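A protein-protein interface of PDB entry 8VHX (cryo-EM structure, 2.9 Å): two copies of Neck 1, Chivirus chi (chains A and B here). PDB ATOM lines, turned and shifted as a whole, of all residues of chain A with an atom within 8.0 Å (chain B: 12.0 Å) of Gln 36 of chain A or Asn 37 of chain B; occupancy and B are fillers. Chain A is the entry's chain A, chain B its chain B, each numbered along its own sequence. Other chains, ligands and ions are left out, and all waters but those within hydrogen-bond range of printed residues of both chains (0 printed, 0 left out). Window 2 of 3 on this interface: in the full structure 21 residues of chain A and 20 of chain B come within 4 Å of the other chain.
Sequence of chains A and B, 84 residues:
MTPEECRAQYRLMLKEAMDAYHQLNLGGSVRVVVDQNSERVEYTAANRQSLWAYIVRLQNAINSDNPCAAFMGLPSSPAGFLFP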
ATOM      1  N   VAL A  33      14.473 -32.313   8.510  1.00  0.00           N
ATOM      2  CA  VAL A  33      14.213 -31.910   9.881  1.00  0.00           C
ATOM      3  C   VAL A  33      13.846 -30.441   9.898  1.00  0.00           C
ATOM      4  O   VAL A  33      14.461 -29.626   9.206  1.00  0.00           O
ATOM      5  CB  VAL A  33      15.417 -32.161  10.792  1.00  0.00           C
ATOM      6  CG1 VAL A  33      15.045 -31.925  12.190  1.00  0.00           C
ATOM      7  CG2 VAL A  33      15.850 -33.536  10.650  1.00  0.00           C
ATOM      8  N   VAL A  34      12.843 -30.110  10.693  1.00  0.00           N
ATOM      9  CA  VAL A  34      12.430 -28.739  10.918  1.00  0.00           C
ATOM     10  C   VAL A  34      12.192 -28.575  12.405  1.00  0.00           C
ATOM     11  O   VAL A  34      11.537 -29.414  13.028  1.00  0.00           O
ATOM     12  CB  VAL A  34      11.166 -28.382  10.123  1.00  0.00           C
ATOM     13  CG1 VAL A  34      10.969 -26.921  10.098  1.00  0.00           C
ATOM     14  CG2 VAL A  34      11.262 -28.891   8.735  1.00  0.00           C
ATOM     15  N   ASP A  35      12.731 -27.512  12.968  1.00  0.00           N
ATOM     16  CA  ASP A  35      12.542 -27.206  14.371  1.00  0.00           C
ATOM     17  C   ASP A  35      11.521 -26.089  14.518  1.00  0.00           C
ATOM     18  O   ASP A  35      11.275 -25.315  13.593  1.00  0.00           O
ATOM     19  CB  ASP A  35      13.870 -26.802  15.001  1.00  0.00           C
ATOM     20  CG  ASP A  35      13.976 -27.208  16.442  1.00  0.00           C
ATOM     21  OD1 ASP A  35      12.932 -27.485  17.066  1.00  0.00           O
ATOM     22  OD2 ASP A  35      15.112 -27.260  16.952  1.00  0.00           O
ATOM     23  N   GLN A  36      10.926 -26.012  15.706  1.00  0.00           N
ATOM     24  CA  GLN A  36      10.028 -24.909  16.007  1.00  0.00           C
ATOM     25  C   GLN A  36      10.732 -23.565  15.917  1.00  0.00           C
ATOM     26  O   GLN A  36      10.062 -22.527  15.903  1.00  0.00           O
ATOM     27  CB  GLN A  36       9.421 -25.128  17.387  1.00  0.00           C
ATOM     28  CG  GLN A  36      10.410 -25.121  18.510  1.00  0.00           C
ATOM     29  CD  GLN A  36       9.893 -25.841  19.722  1.00  0.00           C
ATOM     30  OE1 GLN A  36       8.703 -26.109  19.833  1.00  0.00           O
ATOM     31  NE2 GLN A  36      10.789 -26.186  20.628  1.00  0.00           N
ATOM     32  N   ASN A  37      12.062 -23.564  15.844  1.00  0.00           N
ATOM     33  CA  ASN A  37      12.827 -22.384  15.473  1.00  0.00           C
ATOM     34  C   ASN A  37      12.588 -21.953  14.035  1.00  0.00           C
ATOM     35  O   ASN A  37      13.106 -20.910  13.629  1.00  0.00           O
ATOM     36  CB  ASN A  37      14.307 -22.666  15.662  1.00  0.00           C
ATOM     37  CG  ASN A  37      14.682 -22.835  17.097  1.00  0.00           C
ATOM     38  OD1 ASN A  37      13.942 -23.425  17.878  1.00  0.00           O
ATOM     39  ND2 ASN A  37      15.844 -22.320  17.461  1.00  0.00           N
ATOM     40  N   SER A  38      11.839 -22.733  13.257  1.00  0.00           N
ATOM     41  CA  SER A  38      11.586 -22.456  11.845  1.00  0.00           C
ATOM     42  C   SER A  38      12.841 -22.624  11.003  1.00  0.00           C
ATOM     43  O   SER A  38      12.951 -22.057   9.916  1.00  0.00           O
ATOM     44  CB  SER A  38      11.001 -21.058  11.639  1.00  0.00           C
ATOM     45  OG  SER A  38      10.801 -20.798  10.262  1.00  0.00           O
ATOM     46  N   GLU A  39      13.785 -23.421  11.481  1.00  0.00           N
ATOM     47  CA  GLU A  39      15.002 -23.711  10.749  1.00  0.00           C
ATOM     48  C   GLU A  39      14.992 -25.156  10.283  1.00  0.00           C
ATOM     49  O   GLU A  39      14.550 -26.052  11.004  1.00  0.00           O
ATOM     50  CB  GLU A  39      16.241 -23.419  11.591  1.00  0.00           C
ATOM     51  CG  GLU A  39      16.488 -24.335  12.730  1.00  0.00           C
ATOM     52  CD  GLU A  39      17.673 -23.887  13.548  1.00  0.00           C
ATOM     53  OE1 GLU A  39      17.900 -22.665  13.648  1.00  0.00           O
ATOM     54  OE2 GLU A  39      18.384 -24.750  14.085  1.00  0.00           O
ATOM     55  N   VAL B  33       6.093 -36.440   9.516  1.00  0.00           N
ATOM     56  CA  VAL B  33       5.454 -36.017  10.749  1.00  0.00           C
ATOM     57  C   VAL B  33       5.515 -34.508  10.857  1.00  0.00           C
ATOM     58  O   VAL B  33       6.536 -33.899  10.527  1.00  0.00           O
ATOM     59  CB  VAL B  33       6.111 -36.659  11.974  1.00  0.00           C
ATOM     60  CG1 VAL B  33       5.636 -35.999  13.185  1.00  0.00           C
ATOM     61  CG2 VAL B  33       5.756 -38.075  12.037  1.00  0.00           C
ATOM     62  N   VAL B  34       4.428 -33.911  11.325  1.00  0.00           N
ATOM     63  CA  VAL B  34       4.355 -32.486  11.601  1.00  0.00           C
ATOM     64  C   VAL B  34       3.518 -32.273  12.852  1.00  0.00           C
ATOM     65  O   VAL B  34       2.383 -32.752  12.933  1.00  0.00           O
ATOM     66  CB  VAL B  34       3.767 -31.727  10.406  1.00  0.00           C
ATOM     67  CG1 VAL B  34       3.812 -30.275  10.635  1.00  0.00           C
ATOM     68  CG2 VAL B  34       4.526 -32.058   9.184  1.00  0.00           C
ATOM     69  N   ASP B  35       4.074 -31.555  13.818  1.00  0.00           N
ATOM     70  CA  ASP B  35       3.396 -31.205  15.055  1.00  0.00           C
ATOM     71  C   ASP B  35       2.764 -29.824  14.944  1.00  0.00           C
ATOM     72  O   ASP B  35       3.127 -29.016  14.089  1.00  0.00           O
ATOM     73  CB  ASP B  35       4.382 -31.233  16.222  1.00  0.00           C
ATOM     74  CG  ASP B  35       3.734 -31.607  17.532  1.00  0.00           C
ATOM     75  OD1 ASP B  35       2.494 -31.550  17.624  1.00  0.00           O
ATOM     76  OD2 ASP B  35       4.465 -31.961  18.478  1.00  0.00           O
ATOM     77  N   GLN B  36       1.807 -29.553  15.835  1.00  0.00           N
ATOM     78  CA  GLN B  36       1.207 -28.227  15.854  1.00  0.00           C
ATOM     79  C   GLN B  36       2.209 -27.169  16.287  1.00  0.00           C
ATOM     80  O   GLN B  36       2.035 -25.985  15.980  1.00  0.00           O
ATOM     81  CB  GLN B  36      -0.042 -28.215  16.733  1.00  0.00           C
ATOM     82  CG  GLN B  36       0.105 -28.574  18.177  1.00  0.00           C
ATOM     83  CD  GLN B  36      -0.169 -30.029  18.440  1.00  0.00           C
ATOM     84  OE1 GLN B  36      -0.024 -30.875  17.561  1.00  0.00           O
ATOM     85  NE2 GLN B  36      -0.634 -30.322  19.638  1.00  0.00           N
ATOM     86  N   ASN B  37       3.275 -27.575  16.972  1.00  0.00           N
ATOM     87  CA  ASN B  37       4.439 -26.718  17.166  1.00  0.00           C
ATOM     88  C   ASN B  37       5.175 -26.464  15.857  1.00  0.00           C
ATOM     89  O   ASN B  37       6.181 -25.754  15.858  1.00  0.00           O
ATOM     90  CB  ASN B  37       5.382 -27.349  18.196  1.00  0.00           C
ATOM     91  CG  ASN B  37       4.622 -28.004  19.388  1.00  0.00           C
ATOM     92  OD1 ASN B  37       3.922 -28.993  19.202  1.00  0.00           O
ATOM     93  ND2 ASN B  37       4.758 -27.455  20.591  1.00  0.00           N
ATOM     94  N   SER B  38       4.678 -27.028  14.751  1.00  0.00           N
ATOM     95  CA  SER B  38       5.205 -26.868  13.399  1.00  0.00           C
ATOM     96  C   SER B  38       6.525 -27.583  13.139  1.00  0.00           C
ATOM     97  O   SER B  38       7.050 -27.508  12.025  1.00  0.00           O
ATOM     98  CB  SER B  38       5.385 -25.396  13.072  1.00  0.00           C
ATOM     99  OG  SER B  38       5.471 -25.235  11.670  1.00  0.00           O
ATOM    100  N   GLU B  39       7.074 -28.277  14.129  1.00  0.00           N
ATOM    101  CA  GLU B  39       8.294 -29.023  13.884  1.00  0.00           C
ATOM    102  C   GLU B  39       7.994 -30.284  13.095  1.00  0.00           C
ATOM    103  O   GLU B  39       6.911 -30.861  13.188  1.00  0.00           O
ATOM    104  CB  GLU B  39       9.008 -29.352  15.188  1.00  0.00           C
ATOM    105  CG  GLU B  39       8.231 -30.174  16.155  1.00  0.00           C
ATOM    106  CD  GLU B  39       8.864 -30.198  17.537  1.00  0.00           C
ATOM    107  OE1 GLU B  39       9.969 -29.642  17.697  1.00  0.00           O
ATOM    108  OE2 GLU B  39       8.252 -30.766  18.467  1.00  0.00           O
ATOM    109  N   ARG B  40       8.974 -30.710  12.312  1.00  0.00           N
ATOM    110  CA  ARG B  40       8.750 -31.676  11.256  1.00  0.00           C
ATOM    111  C   ARG B  40       9.903 -32.653  11.183  1.00  0.00           C
ATOM    112  O   ARG B  40      11.046 -32.323  11.496  1.00  0.00           O
ATOM    113  CB  ARG B  40       8.579 -30.991   9.906  1.00  0.00           C
ATOM    114  CG  ARG B  40       8.496 -31.901   8.747  1.00  0.00           C
ATOM    115  CD  ARG B  40       8.500 -31.131   7.470  1.00  0.00           C
ATOM    116  NE  ARG B  40       7.342 -30.253   7.365  1.00  0.00           N
ATOM    117  CZ  ARG B  40       6.400 -30.351   6.433  1.00  0.00           C
ATOM    118  NH1 ARG B  40       5.396 -29.500   6.435  1.00  0.00           N
ATOM    119  NH2 ARG B  40       6.449 -31.296   5.507  1.00  0.00           N
ATOM    120  N   VAL B  41       9.571 -33.864  10.775  1.00  0.00           N
ATOM    121  CA  VAL B  41      10.536 -34.894  10.442  1.00  0.00           C
ATOM    122  C   VAL B  41       9.998 -35.652   9.245  1.00  0.00           C
ATOM    123  O   VAL B  41       8.840 -36.076   9.238  1.00  0.00           O
ATOM    124  CB  VAL B  41      10.786 -35.859  11.611  1.00  0.00           C
ATOM    125  CG1 VAL B  41      11.977 -36.663  11.344  1.00  0.00           C
ATOM    126  CG2 VAL B  41      10.985 -35.123  12.867  1.00  0.00           C
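Gln 36 of chain A touches two residues of chain B.
Of chain A, only Gln 36 comes within 4 Å of Asn 37 of chain B.
Of chain B, only Glu 39 comes within 4 Å of Asp 35 of chain A.
No residue of chain B comes within 4 Å of Ser 38 of chain A.
No residue of chain B comes within 4 Å of Glu 39 of chain A.
Printed residues of chain B within 4 Å of Val 33 of chain A: Arg 40.
Of the printed residues of chain A, Arg 40 of chain B touches Val 33 and Val 34.
Ser 38 of chain B touches none of the printed residues of chain A.
The nearest residue of chain B that does not touch Gln 36 of chain A is Ser 38 of chain B (5.3 Å).
The nearest residue of chain A that does not touch Asn 37 of chain B is Asp 35 of chain A (5.5 Å).
The nearest printed residue of chain B that does not touch Val 33 of chain A is Val 41 of chain B (4.8 Å).
OD2 of Asp 35 of chain B lies close to OD1 of Asn 37 of chain B, 3.1 Å away.
The backbone carbonyl oxygen (O) of Val 34 of chain A sits at hydrogen-bond distance from the backbone NH (N) of Arg 40 of chain B (3.0 Å).
Val 34 of chain A touches Glu 39 of chain B, but with the chains exchanged Glu 39 of chain A does not touch Val 34 of chain B (11.5 Å).
Asp 35 of chain A touches Glu 39 of chain B, but with the chains exchanged Glu 39 of chain A does not touch Asp 35 of chain B (12.2 Å).
Gln 36 of chain A touches Asn 37 of chain B, but with the chains exchanged Asn 37 of chain A does not touch Gln 36 of chain B (10.3 Å).
Gln 36 of chain A touches Glu 39 of chain B, but with the chains exchanged Glu 39 of chain A does not touch Gln 36 of chain B (12.8 Å).
Of the 6 pairs that touch across the chains among the printed residues, none has its exchanged pair printed and touching as well.
Among the printed residues, merely in contact across the chains: Val 34 of chain A with Glu 39 of chain B (3.3 Å), Val 33 of chain A with Arg 40 of chain B (3.6 Å), Gln 36 of chain A with Asn 37 of chain B (3.6 Å), Asp 35 of chain A with Glu 39 of chain B (3.7 Å) and Gln 36 of chain A with Glu 39 of chain B (3.9 Å).
Of the 7 printed residues of chain A, 4 touch a printed residue of chain B.
Hydrophobic or aromatic side chains of chain A that line the printed part of chain B: Val 34.
Among the printed residues, 6 pairs touch across the chains.
Among the printed residues, no Asp or Glu carboxylate lies within 4 Å of a Lys or Arg side-chain nitrogen of the other chain.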
